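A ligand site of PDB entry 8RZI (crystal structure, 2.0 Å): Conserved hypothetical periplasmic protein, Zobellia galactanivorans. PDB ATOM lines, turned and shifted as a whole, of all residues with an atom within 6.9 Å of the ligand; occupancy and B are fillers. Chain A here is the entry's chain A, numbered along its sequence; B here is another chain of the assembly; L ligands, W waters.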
ATOM      1  N   TYR A 325      -7.503  22.128 -13.969  1.00  0.00           N
ATOM      2  CA  TYR A 325      -6.621  22.115 -12.808  1.00  0.00           C
ATOM      3  C   TYR A 325      -5.544  21.057 -13.034  1.00  0.00           C
ATOM      4  O   TYR A 325      -5.807  19.852 -12.910  1.00  0.00           O
ATOM      5  CB  TYR A 325      -7.383  21.876 -11.507  1.00  0.00           C
ATOM      6  CG  TYR A 325      -6.434  21.850 -10.326  1.00  0.00           C
ATOM      7  CD1 TYR A 325      -5.843  23.019  -9.871  1.00  0.00           C
ATOM      8  CD2 TYR A 325      -6.073  20.646  -9.724  1.00  0.00           C
ATOM      9  CE1 TYR A 325      -4.952  23.013  -8.820  1.00  0.00           C
ATOM     10  CE2 TYR A 325      -5.170  20.618  -8.674  1.00  0.00           C
ATOM     11  CZ  TYR A 325      -4.616  21.792  -8.238  1.00  0.00           C
ATOM     12  OH  TYR A 325      -3.719  21.776  -7.206  1.00  0.00           O
ATOM     13  N   TYR A 328      -1.220  22.381 -10.258  1.00  0.00           N
ATOM     14  CA  TYR A 328      -0.467  23.592 -10.052  1.00  0.00           C
ATOM     15  C   TYR A 328      -1.418  24.649  -9.495  1.00  0.00           C
ATOM     16  O   TYR A 328      -2.568  24.718  -9.953  1.00  0.00           O
ATOM     17  CB  TYR A 328       0.119  24.056 -11.405  1.00  0.00           C
ATOM     18  CG  TYR A 328       1.088  25.203 -11.375  1.00  0.00           C
ATOM     19  CD1 TYR A 328       0.636  26.520 -11.470  1.00  0.00           C
ATOM     20  CD2 TYR A 328       2.485  24.970 -11.306  1.00  0.00           C
ATOM     21  CE1 TYR A 328       1.538  27.588 -11.455  1.00  0.00           C
ATOM     22  CE2 TYR A 328       3.390  26.036 -11.305  1.00  0.00           C
ATOM     23  CZ  TYR A 328       2.901  27.342 -11.379  1.00  0.00           C
ATOM     24  OH  TYR A 328       3.778  28.407 -11.386  1.00  0.00           O
ATOM     25  N   PRO A 329      -1.011  25.502  -8.544  1.00  0.00           N
ATOM     26  CA  PRO A 329       0.336  25.802  -8.068  1.00  0.00           C
ATOM     27  C   PRO A 329       0.905  24.844  -7.034  1.00  0.00           C
ATOM     28  O   PRO A 329       2.076  24.992  -6.660  1.00  0.00           O
ATOM     29  CB  PRO A 329       0.164  27.207  -7.460  1.00  0.00           C
ATOM     30  CG  PRO A 329      -1.256  27.184  -6.943  1.00  0.00           C
ATOM     31  CD  PRO A 329      -2.022  26.432  -7.987  1.00  0.00           C
ATOM     32  N   HIS A 330       0.110  23.860  -6.616  1.00  0.00           N
ATOM     33  CA  HIS A 330       0.503  22.987  -5.510  1.00  0.00           C
ATOM     34  C   HIS A 330       1.734  22.166  -5.859  1.00  0.00           C
ATOM     35  O   HIS A 330       2.566  21.887  -4.987  1.00  0.00           O
ATOM     36  CB  HIS A 330      -0.668  22.084  -5.128  1.00  0.00           C
ATOM     37  CG  HIS A 330      -1.847  22.859  -4.632  1.00  0.00           C
ATOM     38  ND1 HIS A 330      -2.606  23.663  -5.460  1.00  0.00           N
ATOM     39  CD2 HIS A 330      -2.323  23.044  -3.376  1.00  0.00           C
ATOM     40  CE1 HIS A 330      -3.531  24.284  -4.746  1.00  0.00           C
ATOM     41  NE2 HIS A 330      -3.379  23.929  -3.477  1.00  0.00           N
ATOM     42  N   TRP A 365      -4.465  25.989 -15.048  1.00  0.00           N
ATOM     43  CA  TRP A 365      -3.685  25.966 -13.818  1.00  0.00           C
ATOM     44  C   TRP A 365      -2.515  25.020 -14.048  1.00  0.00           C
ATOM     45  O   TRP A 365      -2.650  23.800 -13.901  1.00  0.00           O
ATOM     46  CB  TRP A 365      -4.519  25.522 -12.620  1.00  0.00           C
ATOM     47  CG  TRP A 365      -5.627  26.445 -12.236  1.00  0.00           C
ATOM     48  CD1 TRP A 365      -6.497  27.101 -13.068  1.00  0.00           C
ATOM     49  CD2 TRP A 365      -5.994  26.823 -10.902  1.00  0.00           C
ATOM     50  NE1 TRP A 365      -7.377  27.859 -12.338  1.00  0.00           N
ATOM     51  CE2 TRP A 365      -7.100  27.702 -11.009  1.00  0.00           C
ATOM     52  CE3 TRP A 365      -5.492  26.491  -9.626  1.00  0.00           C
ATOM     53  CZ2 TRP A 365      -7.712  28.257  -9.886  1.00  0.00           C
ATOM     54  CZ3 TRP A 365      -6.108  27.022  -8.524  1.00  0.00           C
ATOM     55  CH2 TRP A 365      -7.196  27.911  -8.657  1.00  0.00           C
ATOM     56  N   TYR A 405      -2.922  30.327 -14.545  1.00  0.00           N
ATOM     57  CA  TYR A 405      -2.941  30.569 -13.110  1.00  0.00           C
ATOM     58  C   TYR A 405      -1.765  31.453 -12.725  1.00  0.00           C
ATOM     59  O   TYR A 405      -0.627  31.164 -13.107  1.00  0.00           O
ATOM     60  CB  TYR A 405      -2.882  29.255 -12.310  1.00  0.00           C
ATOM     61  CG  TYR A 405      -2.828  29.498 -10.802  1.00  0.00           C
ATOM     62  CD1 TYR A 405      -1.621  29.795 -10.157  1.00  0.00           C
ATOM     63  CD2 TYR A 405      -3.987  29.468 -10.027  1.00  0.00           C
ATOM     64  CE1 TYR A 405      -1.574  30.052  -8.809  1.00  0.00           C
ATOM     65  CE2 TYR A 405      -3.945  29.699  -8.661  1.00  0.00           C
ATOM     66  CZ  TYR A 405      -2.734  29.996  -8.067  1.00  0.00           C
ATOM     67  OH  TYR A 405      -2.674  30.238  -6.728  1.00  0.00           O
ATOM     68  N   ALA A 407      -0.131  33.762  -9.181  1.00  0.00           N
ATOM     69  CA  ALA A 407      -0.202  34.219  -7.797  1.00  0.00           C
ATOM     70  C   ALA A 407       1.159  34.798  -7.423  1.00  0.00           C
ATOM     71  O   ALA A 407       2.195  34.242  -7.796  1.00  0.00           O
ATOM     72  CB  ALA A 407      -0.593  33.084  -6.845  1.00  0.00           C
ATOM     73  N   PRO A 410       2.191  33.589  -2.586  1.00  0.00           N
ATOM     74  CA  PRO A 410       2.618  32.375  -1.883  1.00  0.00           C
ATOM     75  C   PRO A 410       4.127  32.323  -1.668  1.00  0.00           C
ATOM     76  O   PRO A 410       4.920  32.964  -2.357  1.00  0.00           O
ATOM     77  CB  PRO A 410       2.188  31.233  -2.807  1.00  0.00           C
ATOM     78  CG  PRO A 410       1.209  31.815  -3.726  1.00  0.00           C
ATOM     79  CD  PRO A 410       1.699  33.219  -3.932  1.00  0.00           C
ATOM     80  N   TRP A 438      -0.259  30.283   1.351  1.00  0.00           N
ATOM     81  CA  TRP A 438      -0.628  30.943   0.097  1.00  0.00           C
ATOM     82  C   TRP A 438      -0.531  32.451   0.181  1.00  0.00           C
ATOM     83  O   TRP A 438      -0.566  33.112  -0.855  1.00  0.00           O
ATOM     84  CB  TRP A 438      -2.041  30.512  -0.358  1.00  0.00           C
ATOM     85  CG  TRP A 438      -2.000  29.056  -0.677  1.00  0.00           C
ATOM     86  CD1 TRP A 438      -2.499  28.030   0.059  1.00  0.00           C
ATOM     87  CD2 TRP A 438      -1.290  28.445  -1.779  1.00  0.00           C
ATOM     88  NE1 TRP A 438      -2.185  26.833  -0.516  1.00  0.00           N
ATOM     89  CE2 TRP A 438      -1.440  27.053  -1.642  1.00  0.00           C
ATOM     90  CE3 TRP A 438      -0.552  28.942  -2.856  1.00  0.00           C
ATOM     91  CZ2 TRP A 438      -0.873  26.151  -2.543  1.00  0.00           C
ATOM     92  CZ3 TRP A 438       0.009  28.049  -3.738  1.00  0.00           C
ATOM     93  CH2 TRP A 438      -0.156  26.668  -3.585  1.00  0.00           C
ATOM     94  N   ASP A 469      -4.744  34.834  -8.111  1.00  0.00           N
ATOM     95  CA  ASP A 469      -5.250  34.154  -6.921  1.00  0.00           C
ATOM     96  C   ASP A 469      -4.814  34.899  -5.657  1.00  0.00           C
ATOM     97  O   ASP A 469      -3.782  35.579  -5.641  1.00  0.00           O
ATOM     98  CB  ASP A 469      -4.708  32.705  -6.841  1.00  0.00           C
ATOM     99  CG  ASP A 469      -5.627  31.763  -6.019  1.00  0.00           C
ATOM    100  OD1 ASP A 469      -6.858  31.991  -6.048  1.00  0.00           O
ATOM    101  OD2 ASP A 469      -5.151  30.765  -5.354  1.00  0.00           O
ATOM    102  N   ILE A 470      -5.635  34.764  -4.602  1.00  0.00           N
ATOM    103  CA  ILE A 470      -5.303  35.030  -3.197  1.00  0.00           C
ATOM    104  C   ILE A 470      -5.252  36.509  -2.796  1.00  0.00           C
ATOM    105  O   ILE A 470      -5.892  36.902  -1.823  1.00  0.00           O
ATOM    106  CB  ILE A 470      -3.982  34.356  -2.755  1.00  0.00           C
ATOM    107  CG1 ILE A 470      -4.035  32.831  -2.958  1.00  0.00           C
ATOM    108  CG2 ILE A 470      -3.724  34.648  -1.272  1.00  0.00           C
ATOM    109  CD1 ILE A 470      -2.695  32.243  -3.523  1.00  0.00           C
ATOM    110  N   GLU A 500      -9.508  35.890  -7.392  1.00  0.00           N
ATOM    111  CA  GLU A 500     -10.137  34.979  -6.456  1.00  0.00           C
ATOM    112  C   GLU A 500     -10.951  35.728  -5.403  1.00  0.00           C
ATOM    113  O   GLU A 500     -10.438  36.585  -4.682  1.00  0.00           O
ATOM    114  CB  GLU A 500      -9.096  34.133  -5.743  1.00  0.00           C
ATOM    115  CG  GLU A 500      -9.787  33.104  -4.838  1.00  0.00           C
ATOM    116  CD  GLU A 500      -8.896  32.504  -3.749  1.00  0.00           C
ATOM    117  OE1 GLU A 500      -7.773  33.015  -3.490  1.00  0.00           O
ATOM    118  OE2 GLU A 500      -9.360  31.503  -3.139  1.00  0.00           O
ATOM    119  N   GLU A 514     -13.948  35.325  -8.935  1.00  0.00           N
ATOM    120  CA  GLU A 514     -14.147  33.881  -8.879  1.00  0.00           C
ATOM    121  C   GLU A 514     -14.511  33.539  -7.437  1.00  0.00           C
ATOM    122  O   GLU A 514     -13.648  33.505  -6.546  1.00  0.00           O
ATOM    123  CB  GLU A 514     -12.911  33.119  -9.323  1.00  0.00           C
ATOM    124  CG  GLU A 514     -12.957  31.594  -8.991  1.00  0.00           C
ATOM    125  CD  GLU A 514     -12.081  31.223  -7.789  1.00  0.00           C
ATOM    126  OE1 GLU A 514     -10.941  31.761  -7.701  1.00  0.00           O
ATOM    127  OE2 GLU A 514     -12.503  30.364  -6.966  1.00  0.00           O
ATOM    128  N   LYS A 547     -17.022  29.344  -6.964  1.00  0.00           N
ATOM    129  CA  LYS A 547     -15.682  29.149  -6.398  1.00  0.00           C
ATOM    130  C   LYS A 547     -15.065  27.850  -6.896  1.00  0.00           C
ATOM    131  O   LYS A 547     -15.752  26.828  -7.013  1.00  0.00           O
ATOM    132  CB  LYS A 547     -15.765  29.127  -4.863  1.00  0.00           C
ATOM    133  CG  LYS A 547     -14.411  29.223  -4.104  1.00  0.00           C
ATOM    134  CD  LYS A 547     -13.920  30.694  -4.126  1.00  0.00           C
ATOM    135  CE  LYS A 547     -12.522  30.838  -3.525  1.00  0.00           C
ATOM    136  NZ  LYS A 547     -11.485  30.182  -4.380  1.00  0.00           N
ATOM    137  N   ILE A 548     -13.756  27.866  -7.162  1.00  0.00           N
ATOM    138  CA  ILE A 548     -13.131  26.688  -7.771  1.00  0.00           C
ATOM    139  C   ILE A 548     -13.164  25.479  -6.834  1.00  0.00           C
ATOM    140  O   ILE A 548     -13.212  24.340  -7.304  1.00  0.00           O
ATOM    141  CB  ILE A 548     -11.688  26.995  -8.239  1.00  0.00           C
ATOM    142  CG1 ILE A 548     -10.787  27.441  -7.063  1.00  0.00           C
ATOM    143  CG2 ILE A 548     -11.701  27.990  -9.448  1.00  0.00           C
ATOM    144  CD1 ILE A 548      -9.922  26.302  -6.485  1.00  0.00           C
ATOM    145  N   GLN A 549     -13.112  25.699  -5.502  1.00  0.00           N
ATOM    146  CA  GLN A 549     -13.134  24.560  -4.571  1.00  0.00           C
ATOM    147  C   GLN A 549     -14.525  23.933  -4.459  1.00  0.00           C
ATOM    148  O   GLN A 549     -14.645  22.799  -3.994  1.00  0.00           O
ATOM    149  CB  GLN A 549     -12.679  24.967  -3.167  1.00  0.00           C
ATOM    150  CG  GLN A 549     -11.167  25.189  -2.982  1.00  0.00           C
ATOM    151  CD  GLN A 549     -10.764  26.639  -3.174  1.00  0.00           C
ATOM    152  OE1 GLN A 549     -11.490  27.429  -3.784  1.00  0.00           O
ATOM    153  NE2 GLN A 549      -9.624  27.009  -2.632  1.00  0.00           N
ATOM    154  N   PHE A 578     -14.819  23.155 -12.842  1.00  0.00           N
ATOM    155  CA  PHE A 578     -13.419  23.131 -12.387  1.00  0.00           C
ATOM    156  C   PHE A 578     -13.011  21.685 -12.198  1.00  0.00           C
ATOM    157  O   PHE A 578     -13.561  20.983 -11.335  1.00  0.00           O
ATOM    158  CB  PHE A 578     -13.246  23.894 -11.075  1.00  0.00           C
ATOM    159  CG  PHE A 578     -11.801  24.197 -10.727  1.00  0.00           C
ATOM    160  CD1 PHE A 578     -11.137  25.275 -11.313  1.00  0.00           C
ATOM    161  CD2 PHE A 578     -11.102  23.396  -9.834  1.00  0.00           C
ATOM    162  CE1 PHE A 578      -9.787  25.554 -10.996  1.00  0.00           C
ATOM    163  CE2 PHE A 578      -9.762  23.660  -9.517  1.00  0.00           C
ATOM    164  CZ  PHE A 578      -9.111  24.740 -10.093  1.00  0.00           C
ATOM    165  N   PHE B 180      -8.845  18.694  -4.672  1.00  0.00           N
ATOM    166  CA  PHE B 180      -7.383  18.638  -4.551  1.00  0.00           C
ATOM    167  C   PHE B 180      -6.839  19.859  -3.820  1.00  0.00           C
ATOM    168  O   PHE B 180      -5.983  19.724  -2.932  1.00  0.00           O
ATOM    169  CB  PHE B 180      -6.775  18.510  -5.948  1.00  0.00           C
ATOM    170  CG  PHE B 180      -5.278  18.205  -5.975  1.00  0.00           C
ATOM    171  CD1 PHE B 180      -4.346  19.192  -5.652  1.00  0.00           C
ATOM    172  CD2 PHE B 180      -4.810  16.963  -6.390  1.00  0.00           C
ATOM    173  CE1 PHE B 180      -2.970  18.937  -5.697  1.00  0.00           C
ATOM    174  CE2 PHE B 180      -3.432  16.685  -6.440  1.00  0.00           C
ATOM    175  CZ  PHE B 180      -2.507  17.690  -6.091  1.00  0.00           C
ATOM    176  N   CYS B 181      -7.323  21.050  -4.166  1.00  0.00           N
ATOM    177  CA  CYS B 181      -6.858  22.251  -3.484  1.00  0.00           C
ATOM    178  C   CYS B 181      -7.158  22.186  -1.989  1.00  0.00           C
ATOM    179  O   CYS B 181      -6.282  22.464  -1.160  1.00  0.00           O
ATOM    180  CB  CYS B 181      -7.472  23.521  -4.115  1.00  0.00           C
ATOM    181  SG  CYS B 181      -6.887  23.868  -5.755  1.00  0.00           S
ATOM    182  N   LYS B 182      -8.395  21.824  -1.625  1.00  0.00           N
ATOM    183  CA  LYS B 182      -8.734  21.735  -0.211  1.00  0.00           C
ATOM    184  C   LYS B 182      -7.920  20.646   0.472  1.00  0.00           C
ATOM    185  O   LYS B 182      -7.481  20.817   1.609  1.00  0.00           O
ATOM    186  CB  LYS B 182     -10.232  21.425  -0.032  1.00  0.00           C
ATOM    187  CG  LYS B 182     -11.192  22.546  -0.494  1.00  0.00           C
ATOM    188  CD  LYS B 182     -12.635  22.157  -0.207  1.00  0.00           C
ATOM    189  CE  LYS B 182     -13.193  21.183  -1.280  1.00  0.00           C
ATOM    190  NZ  LYS B 182     -14.658  20.856  -1.067  1.00  0.00           N
ATOM    191  N   ASP B 185      -4.129  21.779   0.769  1.00  0.00           N
ATOM    192  CA  ASP B 185      -4.045  22.925   1.670  1.00  0.00           C
ATOM    193  C   ASP B 185      -4.243  22.501   3.118  1.00  0.00           C
ATOM    194  O   ASP B 185      -3.582  23.037   4.029  1.00  0.00           O
ATOM    195  CB  ASP B 185      -5.087  23.972   1.285  1.00  0.00           C
ATOM    196  CG  ASP B 185      -4.744  24.667  -0.028  1.00  0.00           C
ATOM    197  OD1 ASP B 185      -3.708  24.322  -0.638  1.00  0.00           O
ATOM    198  OD2 ASP B 185      -5.543  25.561  -0.457  1.00  0.00           O
HETATM  199  C1  LIG L   1      -5.827  30.060  -4.749  1.00  0.00           C
HETATM  200  C2  LIG L   1      -6.670  28.983  -5.198  1.00  0.00           C
HETATM  201  C3  LIG L   1      -5.957  27.690  -4.885  1.00  0.00           C
HETATM  202  C4  LIG L   1      -5.844  27.584  -3.417  1.00  0.00           C
HETATM  203  C5  LIG L   1      -4.776  28.590  -3.250  1.00  0.00           C
HETATM  204  C6  LIG L   1      -3.866  28.135  -4.332  1.00  0.00           C
HETATM  205  F1  LIG L   1      -7.721  28.928  -4.700  1.00  0.00           F
HETATM  206  O1  LIG L   1      -5.241  29.872  -3.558  1.00  0.00           O
HETATM  207  O2  LIG L   1      -4.663  27.769  -5.326  1.00  0.00           O
HETATM  208  O3  LIG L   1      -5.486  26.271  -3.096  1.00  0.00           O
HETATM  209  O   HOH W   1      -8.676  29.684  -1.531  1.00  0.00           O
HETATM  210  O   HOH W   2      -8.707  30.570  -7.413  1.00  0.00           O
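A carbon (C1) of the ligand is bonded to the side-chain carboxylate (OD2) of Asp 469 (1.1 Å). OD2 of Asp 185 of chain B lies within hydrogen-bond range of O3 of the ligand (2.7 Å). NE2 of His 330 is in hydrogen-bond range of O3 of the ligand, at 3.2 Å. O2 of the ligand lies close to OH of Tyr 405 (3.5 Å).
The side-chain carboxylate (OD2) of Asp 469 lies within hydrogen-bond range of the side-chain hydroxyl (OH) of Tyr 405 (2.9 Å). The side-chain carboxylate of Asp 185 of chain B lies within hydrogen-bond range of the indole nitrogen of Trp 438, 2.9 Å away. A ring nitrogen (ND1) of His 330 is in hydrogen-bond range of the side-chain hydroxyl (OH) of Tyr 325, 2.8 Å away. N of Ile 470 is in hydrogen-bond range of OE1 of Glu 500 (3.0 Å). OE1 of Gln 549 is in hydrogen-bond range of NZ of Lys 547 (2.8 Å). OE2 of Glu 500 lies within salt-bridge range of NZ of Lys 547 (2.8 Å). The side-chain carboxylate (OE2) of Glu 514 is in hydrogen-bond range of the backbone NH (N) of Ile 548 (2.8 Å). The side-chain amino group (NZ) of Lys 547 is in salt-bridge range of the side-chain carboxylate (OE2) of Glu 514, 2.8 Å away.
F1 of the ligand lies close to OE2 of Glu 500, at 3.4 Å. The side-chain amide nitrogen (NE2) of Gln 549 sits close to a fluorine (F1) of the ligand. Merely in contact with the ligand: Ile 470, Cys 181 of chain B, Trp 365, Trp 438, Pro 329, Ile 548 and Lys 547. Within 4 Å of the ligand: Pro 329, His 330, Trp 365, Tyr 405, Trp 438, Asp 469, Ile 470, Glu 500, Lys 547, Ile 548, Gln 549, Cys 181 of chain B and Asp 185 of chain B. The nearest printed residue that does not touch the ligand is Glu 514 (5.2 Å).
Water W2 bridges OE1 of Glu 514 and OD1 of Asp 469. Water W1 bridges OE2 of Glu 500 and NE2 of Gln 549.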
